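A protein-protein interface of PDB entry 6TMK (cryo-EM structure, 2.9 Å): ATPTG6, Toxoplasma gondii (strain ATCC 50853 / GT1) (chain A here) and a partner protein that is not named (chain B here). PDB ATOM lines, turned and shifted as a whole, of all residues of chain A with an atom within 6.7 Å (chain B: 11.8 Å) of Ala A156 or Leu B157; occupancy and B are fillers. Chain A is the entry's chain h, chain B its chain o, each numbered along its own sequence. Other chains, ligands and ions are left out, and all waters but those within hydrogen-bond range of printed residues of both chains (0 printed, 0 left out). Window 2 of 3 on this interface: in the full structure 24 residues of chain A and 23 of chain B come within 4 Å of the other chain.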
ATOM      1  N   ALA A 151     -23.323 -15.710  -3.606  1.00  0.00           N
ATOM      2  CA  ALA A 151     -22.067 -14.978  -3.652  1.00  0.00           C
ATOM      3  C   ALA A 151     -22.143 -13.702  -2.825  1.00  0.00           C
ATOM      4  O   ALA A 151     -21.236 -13.396  -2.041  1.00  0.00           O
ATOM      5  CB  ALA A 151     -21.723 -14.661  -5.103  1.00  0.00           C
ATOM      6  N   VAL A 152     -23.228 -12.945  -2.988  1.00  0.00           N
ATOM      7  CA  VAL A 152     -23.360 -11.677  -2.286  1.00  0.00           C
ATOM      8  C   VAL A 152     -23.403 -11.896  -0.784  1.00  0.00           C
ATOM      9  O   VAL A 152     -22.794 -11.143  -0.017  1.00  0.00           O
ATOM     10  CB  VAL A 152     -24.612 -10.932  -2.775  1.00  0.00           C
ATOM     11  CG1 VAL A 152     -24.911  -9.761  -1.882  1.00  0.00           C
ATOM     12  CG2 VAL A 152     -24.440 -10.482  -4.201  1.00  0.00           C
ATOM     13  N   ASN A 153     -24.112 -12.929  -0.335  1.00  0.00           N
ATOM     14  CA  ASN A 153     -24.250 -13.146   1.097  1.00  0.00           C
ATOM     15  C   ASN A 153     -22.947 -13.633   1.711  1.00  0.00           C
ATOM     16  O   ASN A 153     -22.599 -13.239   2.830  1.00  0.00           O
ATOM     17  CB  ASN A 153     -25.394 -14.117   1.362  1.00  0.00           C
ATOM     18  CG  ASN A 153     -26.728 -13.573   0.907  1.00  0.00           C
ATOM     19  OD1 ASN A 153     -26.970 -12.371   0.958  1.00  0.00           O
ATOM     20  ND2 ASN A 153     -27.603 -14.455   0.470  1.00  0.00           N
ATOM     21  N   ASP A 154     -22.198 -14.468   0.990  1.00  0.00           N
ATOM     22  CA  ASP A 154     -20.883 -14.868   1.473  1.00  0.00           C
ATOM     23  C   ASP A 154     -19.953 -13.665   1.586  1.00  0.00           C
ATOM     24  O   ASP A 154     -19.244 -13.496   2.588  1.00  0.00           O
ATOM     25  CB  ASP A 154     -20.291 -15.928   0.546  1.00  0.00           C
ATOM     26  CG  ASP A 154     -20.797 -17.324   0.858  1.00  0.00           C
ATOM     27  OD1 ASP A 154     -20.294 -17.938   1.824  1.00  0.00           O
ATOM     28  OD2 ASP A 154     -21.699 -17.809   0.141  1.00  0.00           O
ATOM     29  N   PHE A 155     -19.945 -12.814   0.558  1.00  0.00           N
ATOM     30  CA  PHE A 155     -19.109 -11.620   0.589  1.00  0.00           C
ATOM     31  C   PHE A 155     -19.508 -10.698   1.735  1.00  0.00           C
ATOM     32  O   PHE A 155     -18.647 -10.123   2.411  1.00  0.00           O
ATOM     33  CB  PHE A 155     -19.206 -10.903  -0.758  1.00  0.00           C
ATOM     34  CG  PHE A 155     -18.433  -9.631  -0.832  1.00  0.00           C
ATOM     35  CD1 PHE A 155     -17.071  -9.648  -1.020  1.00  0.00           C
ATOM     36  CD2 PHE A 155     -19.070  -8.418  -0.723  1.00  0.00           C
ATOM     37  CE1 PHE A 155     -16.363  -8.483  -1.089  1.00  0.00           C
ATOM     38  CE2 PHE A 155     -18.365  -7.252  -0.792  1.00  0.00           C
ATOM     39  CZ  PHE A 155     -17.012  -7.281  -0.976  1.00  0.00           C
ATOM     40  N   ALA A 156     -20.811 -10.546   1.968  1.00  0.00           N
ATOM     41  CA  ALA A 156     -21.283  -9.707   3.059  1.00  0.00           C
ATOM     42  C   ALA A 156     -20.842 -10.255   4.406  1.00  0.00           C
ATOM     43  O   ALA A 156     -20.444  -9.495   5.296  1.00  0.00           O
ATOM     44  CB  ALA A 156     -22.799  -9.590   2.997  1.00  0.00           C
ATOM     45  N   ALA A 157     -20.924 -11.573   4.583  1.00  0.00           N
ATOM     46  CA  ALA A 157     -20.453 -12.179   5.820  1.00  0.00           C
ATOM     47  C   ALA A 157     -18.969 -11.912   6.027  1.00  0.00           C
ATOM     48  O   ALA A 157     -18.539 -11.558   7.132  1.00  0.00           O
ATOM     49  CB  ALA A 157     -20.736 -13.675   5.800  1.00  0.00           C
ATOM     50  N   LYS A 158     -18.171 -12.081   4.972  1.00  0.00           N
ATOM     51  CA  LYS A 158     -16.736 -11.851   5.095  1.00  0.00           C
ATOM     52  C   LYS A 158     -16.436 -10.398   5.438  1.00  0.00           C
ATOM     53  O   LYS A 158     -15.539 -10.113   6.237  1.00  0.00           O
ATOM     54  CB  LYS A 158     -16.027 -12.259   3.808  1.00  0.00           C
ATOM     55  CG  LYS A 158     -16.075 -13.743   3.537  1.00  0.00           C
ATOM     56  CD  LYS A 158     -15.460 -14.098   2.206  1.00  0.00           C
ATOM     57  CE  LYS A 158     -15.633 -15.574   1.911  1.00  0.00           C
ATOM     58  NZ  LYS A 158     -16.247 -15.833   0.585  1.00  0.00           N
ATOM     59  N   VAL A 159     -17.194  -9.466   4.867  1.00  0.00           N
ATOM     60  CA  VAL A 159     -16.937  -8.054   5.130  1.00  0.00           C
ATOM     61  C   VAL A 159     -17.331  -7.699   6.558  1.00  0.00           C
ATOM     62  O   VAL A 159     -16.618  -6.962   7.256  1.00  0.00           O
ATOM     63  CB  VAL A 159     -17.691  -7.192   4.102  1.00  0.00           C
ATOM     64  CG1 VAL A 159     -17.737  -5.757   4.535  1.00  0.00           C
ATOM     65  CG2 VAL A 159     -17.046  -7.301   2.755  1.00  0.00           C
ATOM     66  N   HIS A 160     -18.470  -8.218   7.011  1.00  0.00           N
ATOM     67  CA  HIS A 160     -18.895  -7.997   8.385  1.00  0.00           C
ATOM     68  C   HIS A 160     -17.879  -8.551   9.370  1.00  0.00           C
ATOM     69  O   HIS A 160     -17.622  -7.947  10.417  1.00  0.00           O
ATOM     70  CB  HIS A 160     -20.256  -8.643   8.607  1.00  0.00           C
ATOM     71  CG  HIS A 160     -20.926  -8.221   9.871  1.00  0.00           C
ATOM     72  ND1 HIS A 160     -21.136  -6.899  10.194  1.00  0.00           N
ATOM     73  CD2 HIS A 160     -21.427  -8.945  10.898  1.00  0.00           C
ATOM     74  CE1 HIS A 160     -21.747  -6.827  11.362  1.00  0.00           C
ATOM     75  NE2 HIS A 160     -21.934  -8.055  11.811  1.00  0.00           N
ATOM     76  N   ALA A 161     -17.294  -9.707   9.056  1.00  0.00           N
ATOM     77  CA  ALA A 161     -16.235 -10.246   9.899  1.00  0.00           C
ATOM     78  C   ALA A 161     -14.988  -9.376   9.849  1.00  0.00           C
ATOM     79  O   ALA A 161     -14.302  -9.209  10.862  1.00  0.00           O
ATOM     80  CB  ALA A 161     -15.904 -11.670   9.467  1.00  0.00           C
ATOM     81  N   LYS A 169     -19.290  -0.262   4.734  1.00  0.00           N
ATOM     82  CA  LYS A 169     -19.561  -1.688   4.612  1.00  0.00           C
ATOM     83  C   LYS A 169     -20.608  -1.973   3.544  1.00  0.00           C
ATOM     84  O   LYS A 169     -20.352  -2.686   2.562  1.00  0.00           O
ATOM     85  CB  LYS A 169     -20.008  -2.204   5.976  1.00  0.00           C
ATOM     86  CG  LYS A 169     -20.490  -3.608   6.019  1.00  0.00           C
ATOM     87  CD  LYS A 169     -20.453  -4.125   7.427  1.00  0.00           C
ATOM     88  CE  LYS A 169     -21.408  -3.351   8.301  1.00  0.00           C
ATOM     89  NZ  LYS A 169     -21.681  -4.021   9.589  1.00  0.00           N
ATOM     90  N   TYR A 170     -21.813  -1.449   3.740  1.00  0.00           N
ATOM     91  CA  TYR A 170     -22.903  -1.733   2.826  1.00  0.00           C
ATOM     92  C   TYR A 170     -22.655  -1.141   1.450  1.00  0.00           C
ATOM     93  O   TYR A 170     -23.187  -1.654   0.465  1.00  0.00           O
ATOM     94  CB  TYR A 170     -24.213  -1.210   3.408  1.00  0.00           C
ATOM     95  CG  TYR A 170     -24.752  -2.058   4.530  1.00  0.00           C
ATOM     96  CD1 TYR A 170     -25.511  -3.184   4.273  1.00  0.00           C
ATOM     97  CD2 TYR A 170     -24.502  -1.731   5.850  1.00  0.00           C
ATOM     98  CE1 TYR A 170     -26.002  -3.956   5.295  1.00  0.00           C
ATOM     99  CE2 TYR A 170     -24.987  -2.499   6.875  1.00  0.00           C
ATOM    100  CZ  TYR A 170     -25.736  -3.609   6.595  1.00  0.00           C
ATOM    101  OH  TYR A 170     -26.225  -4.379   7.620  1.00  0.00           O
ATOM    102  N   ILE A 173     -20.597  -3.740  -0.232  1.00  0.00           N
ATOM    103  CA  ILE A 173     -21.508  -4.836  -0.551  1.00  0.00           C
ATOM    104  C   ILE A 173     -22.367  -4.490  -1.760  1.00  0.00           C
ATOM    105  O   ILE A 173     -22.677  -5.355  -2.585  1.00  0.00           O
ATOM    106  CB  ILE A 173     -22.370  -5.191   0.674  1.00  0.00           C
ATOM    107  CG1 ILE A 173     -21.519  -5.858   1.742  1.00  0.00           C
ATOM    108  CG2 ILE A 173     -23.481  -6.129   0.295  1.00  0.00           C
ATOM    109  CD1 ILE A 173     -22.033  -5.681   3.132  1.00  0.00           C
ATOM    110  N   PHE A 176     -20.361  -4.795  -5.030  1.00  0.00           N
ATOM    111  CA  PHE A 176     -20.253  -6.216  -5.340  1.00  0.00           C
ATOM    112  C   PHE A 176     -21.559  -6.750  -5.921  1.00  0.00           C
ATOM    113  O   PHE A 176     -21.568  -7.466  -6.932  1.00  0.00           O
ATOM    114  CB  PHE A 176     -19.879  -6.982  -4.075  1.00  0.00           C
ATOM    115  CG  PHE A 176     -19.558  -8.419  -4.303  1.00  0.00           C
ATOM    116  CD1 PHE A 176     -18.276  -8.812  -4.597  1.00  0.00           C
ATOM    117  CD2 PHE A 176     -20.538  -9.378  -4.222  1.00  0.00           C
ATOM    118  CE1 PHE A 176     -17.980 -10.128  -4.802  1.00  0.00           C
ATOM    119  CE2 PHE A 176     -20.241 -10.695  -4.432  1.00  0.00           C
ATOM    120  CZ  PHE A 176     -18.966 -11.068  -4.723  1.00  0.00           C
ATOM    121  N   ASN B  73     -36.713   1.301   7.757  1.00  0.00           N
ATOM    122  CA  ASN B  73     -36.619   0.379   6.631  1.00  0.00           C
ATOM    123  C   ASN B  73     -37.856  -0.502   6.523  1.00  0.00           C
ATOM    124  O   ASN B  73     -38.421  -0.663   5.435  1.00  0.00           O
ATOM    125  CB  ASN B  73     -35.364  -0.479   6.787  1.00  0.00           C
ATOM    126  CG  ASN B  73     -34.896  -1.080   5.488  1.00  0.00           C
ATOM    127  OD1 ASN B  73     -35.015  -2.283   5.272  1.00  0.00           O
ATOM    128  ND2 ASN B  73     -34.344  -0.252   4.618  1.00  0.00           N
ATOM    129  N   GLU B  74     -38.289  -1.085   7.637  1.00  0.00           N
ATOM    130  CA  GLU B  74     -39.318  -2.108   7.634  1.00  0.00           C
ATOM    131  C   GLU B  74     -40.440  -1.733   8.588  1.00  0.00           C
ATOM    132  O   GLU B  74     -40.229  -1.023   9.574  1.00  0.00           O
ATOM    133  CB  GLU B  74     -38.736  -3.463   8.029  1.00  0.00           C
ATOM    134  CG  GLU B  74     -37.929  -4.126   6.933  1.00  0.00           C
ATOM    135  CD  GLU B  74     -36.986  -5.190   7.456  1.00  0.00           C
ATOM    136  OE1 GLU B  74     -36.821  -5.293   8.689  1.00  0.00           O
ATOM    137  OE2 GLU B  74     -36.406  -5.927   6.631  1.00  0.00           O
ATOM    138  N   LYS B  76     -41.983  -3.800  10.510  1.00  0.00           N
ATOM    139  CA  LYS B  76     -41.806  -4.527  11.759  1.00  0.00           C
ATOM    140  C   LYS B  76     -40.967  -3.750  12.763  1.00  0.00           C
ATOM    141  O   LYS B  76     -41.065  -4.009  13.966  1.00  0.00           O
ATOM    142  CB  LYS B  76     -41.179  -5.891  11.487  1.00  0.00           C
ATOM    143  CG  LYS B  76     -39.671  -5.911  11.517  1.00  0.00           C
ATOM    144  CD  LYS B  76     -39.133  -7.143  10.813  1.00  0.00           C
ATOM    145  CE  LYS B  76     -37.647  -7.306  11.038  1.00  0.00           C
ATOM    146  NZ  LYS B  76     -37.331  -7.724  12.427  1.00  0.00           N
ATOM    147  N   LEU B  77     -40.148  -2.814  12.297  1.00  0.00           N
ATOM    148  CA  LEU B  77     -39.340  -1.973  13.164  1.00  0.00           C
ATOM    149  C   LEU B  77     -40.067  -0.715  13.613  1.00  0.00           C
ATOM    150  O   LEU B  77     -39.502   0.065  14.384  1.00  0.00           O
ATOM    151  CB  LEU B  77     -38.046  -1.577  12.460  1.00  0.00           C
ATOM    152  CG  LEU B  77     -37.099  -2.713  12.108  1.00  0.00           C
ATOM    153  CD1 LEU B  77     -36.064  -2.198  11.154  1.00  0.00           C
ATOM    154  CD2 LEU B  77     -36.444  -3.278  13.346  1.00  0.00           C
ATOM    155  N   GLU B 119     -33.420  -5.471  18.104  1.00  0.00           N
ATOM    156  CA  GLU B 119     -32.020  -5.827  18.258  1.00  0.00           C
ATOM    157  C   GLU B 119     -31.230  -5.415  17.025  1.00  0.00           C
ATOM    158  O   GLU B 119     -31.711  -5.534  15.895  1.00  0.00           O
ATOM    159  CB  GLU B 119     -31.859  -7.327  18.510  1.00  0.00           C
ATOM    160  CG  GLU B 119     -32.531  -8.216  17.480  1.00  0.00           C
ATOM    161  CD  GLU B 119     -33.972  -8.536  17.835  1.00  0.00           C
ATOM    162  OE1 GLU B 119     -34.589  -9.358  17.125  1.00  0.00           O
ATOM    163  OE2 GLU B 119     -34.488  -7.966  18.819  1.00  0.00           O
ATOM    164  N   ASN B 120     -30.017  -4.922  17.256  1.00  0.00           N
ATOM    165  CA  ASN B 120     -29.095  -4.573  16.181  1.00  0.00           C
ATOM    166  C   ASN B 120     -29.685  -3.502  15.270  1.00  0.00           C
ATOM    167  O   ASN B 120     -29.525  -3.539  14.049  1.00  0.00           O
ATOM    168  CB  ASN B 120     -28.710  -5.815  15.377  1.00  0.00           C
ATOM    169  CG  ASN B 120     -28.282  -6.966  16.257  1.00  0.00           C
ATOM    170  OD1 ASN B 120     -27.464  -6.801  17.161  1.00  0.00           O
ATOM    171  ND2 ASN B 120     -28.839  -8.142  15.999  1.00  0.00           N
ATOM    172  N   VAL B 121     -30.376  -2.541  15.867  1.00  0.00           N
ATOM    173  CA  VAL B 121     -30.908  -1.408  15.122  1.00  0.00           C
ATOM    174  C   VAL B 121     -29.821  -0.354  14.987  1.00  0.00           C
ATOM    175  O   VAL B 121     -29.112  -0.040  15.950  1.00  0.00           O
ATOM    176  CB  VAL B 121     -32.159  -0.836  15.811  1.00  0.00           C
ATOM    177  CG1 VAL B 121     -32.526   0.491  15.208  1.00  0.00           C
ATOM    178  CG2 VAL B 121     -33.311  -1.778  15.664  1.00  0.00           C
ATOM    179  N   LYS B 122     -29.686   0.196  13.786  1.00  0.00           N
ATOM    180  CA  LYS B 122     -28.647   1.166  13.495  1.00  0.00           C
ATOM    181  C   LYS B 122     -29.191   2.252  12.584  1.00  0.00           C
ATOM    182  O   LYS B 122     -30.236   2.099  11.943  1.00  0.00           O
ATOM    183  CB  LYS B 122     -27.420   0.500  12.866  1.00  0.00           C
ATOM    184  CG  LYS B 122     -26.702  -0.439  13.797  1.00  0.00           C
ATOM    185  CD  LYS B 122     -25.338  -0.808  13.285  1.00  0.00           C
ATOM    186  CE  LYS B 122     -24.508  -1.436  14.380  1.00  0.00           C
ATOM    187  NZ  LYS B 122     -25.187  -2.607  14.994  1.00  0.00           N
ATOM    188  N   GLY B 127     -26.253   5.911   3.010  1.00  0.00           N
ATOM    189  CA  GLY B 127     -25.601   4.627   2.939  1.00  0.00           C
ATOM    190  C   GLY B 127     -24.522   4.384   3.965  1.00  0.00           C
ATOM    191  O   GLY B 127     -23.844   3.353   3.890  1.00  0.00           O
ATOM    192  N   VAL B 129     -23.236   4.020   7.858  1.00  0.00           N
ATOM    193  CA  VAL B 129     -23.716   3.614   9.167  1.00  0.00           C
ATOM    194  C   VAL B 129     -23.056   4.462  10.240  1.00  0.00           C
ATOM    195  O   VAL B 129     -21.854   4.744  10.191  1.00  0.00           O
ATOM    196  CB  VAL B 129     -23.456   2.118   9.393  1.00  0.00           C
ATOM    197  CG1 VAL B 129     -24.075   1.673  10.689  1.00  0.00           C
ATOM    198  CG2 VAL B 129     -24.004   1.323   8.247  1.00  0.00           C
ATOM    199  N   PHE B 153     -32.437   0.944  10.369  1.00  0.00           N
ATOM    200  CA  PHE B 153     -32.480  -0.383   9.781  1.00  0.00           C
ATOM    201  C   PHE B 153     -31.952  -1.391  10.789  1.00  0.00           C
ATOM    202  O   PHE B 153     -31.409  -1.031  11.834  1.00  0.00           O
ATOM    203  CB  PHE B 153     -31.689  -0.426   8.468  1.00  0.00           C
ATOM    204  CG  PHE B 153     -30.220  -0.277   8.644  1.00  0.00           C
ATOM    205  CD1 PHE B 153     -29.660   0.965   8.835  1.00  0.00           C
ATOM    206  CD2 PHE B 153     -29.392  -1.375   8.610  1.00  0.00           C
ATOM    207  CE1 PHE B 153     -28.316   1.102   9.002  1.00  0.00           C
ATOM    208  CE2 PHE B 153     -28.046  -1.234   8.774  1.00  0.00           C
ATOM    209  CZ  PHE B 153     -27.509   0.006   8.968  1.00  0.00           C
ATOM    210  N   GLN B 154     -32.148  -2.670  10.485  1.00  0.00           N
ATOM    211  CA  GLN B 154     -31.663  -3.756  11.322  1.00  0.00           C
ATOM    212  C   GLN B 154     -30.381  -4.305  10.713  1.00  0.00           C
ATOM    213  O   GLN B 154     -30.371  -4.716   9.548  1.00  0.00           O
ATOM    214  CB  GLN B 154     -32.717  -4.851  11.454  1.00  0.00           C
ATOM    215  CG  GLN B 154     -32.771  -5.496  12.818  1.00  0.00           C
ATOM    216  CD  GLN B 154     -33.826  -6.566  12.918  1.00  0.00           C
ATOM    217  OE1 GLN B 154     -34.339  -7.049  11.910  1.00  0.00           O
ATOM    218  NE2 GLN B 154     -34.163  -6.942  14.140  1.00  0.00           N
ATOM    219  N   ASP B 155     -29.306  -4.307  11.495  1.00  0.00           N
ATOM    220  CA  ASP B 155     -27.991  -4.744  11.030  1.00  0.00           C
ATOM    221  C   ASP B 155     -27.720  -6.143  11.571  1.00  0.00           C
ATOM    222  O   ASP B 155     -27.087  -6.313  12.614  1.00  0.00           O
ATOM    223  CB  ASP B 155     -26.911  -3.763  11.462  1.00  0.00           C
ATOM    224  CG  ASP B 155     -25.578  -4.032  10.793  1.00  0.00           C
ATOM    225  OD1 ASP B 155     -25.044  -5.149  10.954  1.00  0.00           O
ATOM    226  OD2 ASP B 155     -25.062  -3.129  10.104  1.00  0.00           O
ATOM    227  N   ASN B 156     -28.200  -7.156  10.853  1.00  0.00           N
ATOM    228  CA  ASN B 156     -27.902  -8.536  11.213  1.00  0.00           C
ATOM    229  C   ASN B 156     -26.667  -9.029  10.471  1.00  0.00           C
ATOM    230  O   ASN B 156     -25.644  -9.345  11.085  1.00  0.00           O
ATOM    231  CB  ASN B 156     -29.106  -9.425  10.894  1.00  0.00           C
ATOM    232  CG  ASN B 156     -30.389  -8.889  11.471  1.00  0.00           C
ATOM    233  OD1 ASN B 156     -30.560  -8.827  12.687  1.00  0.00           O
ATOM    234  ND2 ASN B 156     -31.302  -8.486  10.598  1.00  0.00           N
ATOM    235  N   LEU B 157     -26.752  -9.075   9.148  1.00  0.00           N
ATOM    236  CA  LEU B 157     -25.612  -9.373   8.296  1.00  0.00           C
ATOM    237  C   LEU B 157     -24.857 -10.623   8.745  1.00  0.00           C
ATOM    238  O   LEU B 157     -23.738 -10.880   8.299  1.00  0.00           O
ATOM    239  CB  LEU B 157     -24.676  -8.170   8.258  1.00  0.00           C
ATOM    240  CG  LEU B 157     -23.881  -7.968   6.971  1.00  0.00           C
ATOM    241  CD1 LEU B 157     -24.796  -7.866   5.767  1.00  0.00           C
ATOM    242  CD2 LEU B 157     -23.045  -6.720   7.081  1.00  0.00           C
ATOM    243  OXT LEU B 157     -25.342 -11.405   9.564  1.00  0.00           O
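Leu B157 touches Ala A156.
His A160 touches Asp B155 (CE1 to OD1, 3.7 Å).
O of Asn B156 touches NE2 of His A160, 3.99 Å away.
His A160 touches Leu B157.
CD of Lys A169 touches CD2 of Leu B157, 3.7 Å away.
CD2 of Tyr A170 touches CG2 of Val B129, at 3.9 Å.
Phe B153 touches Tyr A170 (CE2 to OH, 3.8 Å).
CD2 of Leu B157 touches OH of Tyr A170, 3.99 Å away.
Of chain B, only Leu B157 (3.8 Å) comes within 4 Å of Ala A156.
Of the printed residues of chain A, Leu B157 touches Ala A156 (3.8 Å), His A160 (3.7 Å), Lys A169 (3.7 Å) and Tyr A170 (3.99 Å).
No residue of chain B comes within 4 Å of Val A152.
Asn A153 touches none of the printed residues of chain B.
No residue of chain B comes within 4 Å of Asp A154.
No residue of chain B comes within 4 Å of Ala A157.
No residue of chain B comes within 4 Å of Lys A158.
No residue of chain B comes within 4 Å of Ile A173.
Of the printed residues of chain B, Lys A169 touches Asp B155 and Leu B157.
Of the printed residues of chain A, Asp B155 touches His A160, Lys A169 and Tyr A170.
The nearest printed residue of chain B that does not touch Lys A169 is Val B129 (5.3 Å).
Of the 15 printed residues of chain A, 4 touch a printed residue of chain B.
Of the 15 printed residues of chain B, 5 touch a printed residue of chain A.
Printed residues of chain B that touch a printed residue of chain A: Val B129, Phe B153, Asp B155, Asn B156 and Leu B157.
Hydrophobic or aromatic side chains of chain B within 4 Å of the printed part of chain A: Val B129, Phe B153 and Leu B157.
The backbone carbonyl oxygen of Asn B120 is in hydrogen-bond range of the backbone NH of Asp B155.
A ring nitrogen (ND1) of His A160 is in hydrogen-bond range of the side-chain amino group (NZ) of Lys A169 (3.0 Å).
The backbone NH of Lys B122 is in hydrogen-bond range of the backbone carbonyl oxygen of Phe B153.
NZ of Lys A169 is in salt-bridge range of OD2 of Asp B155, 3.5 Å away.
OH of Tyr A170 lies within hydrogen-bond range of OD2 of Asp B155 (3.0 Å).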
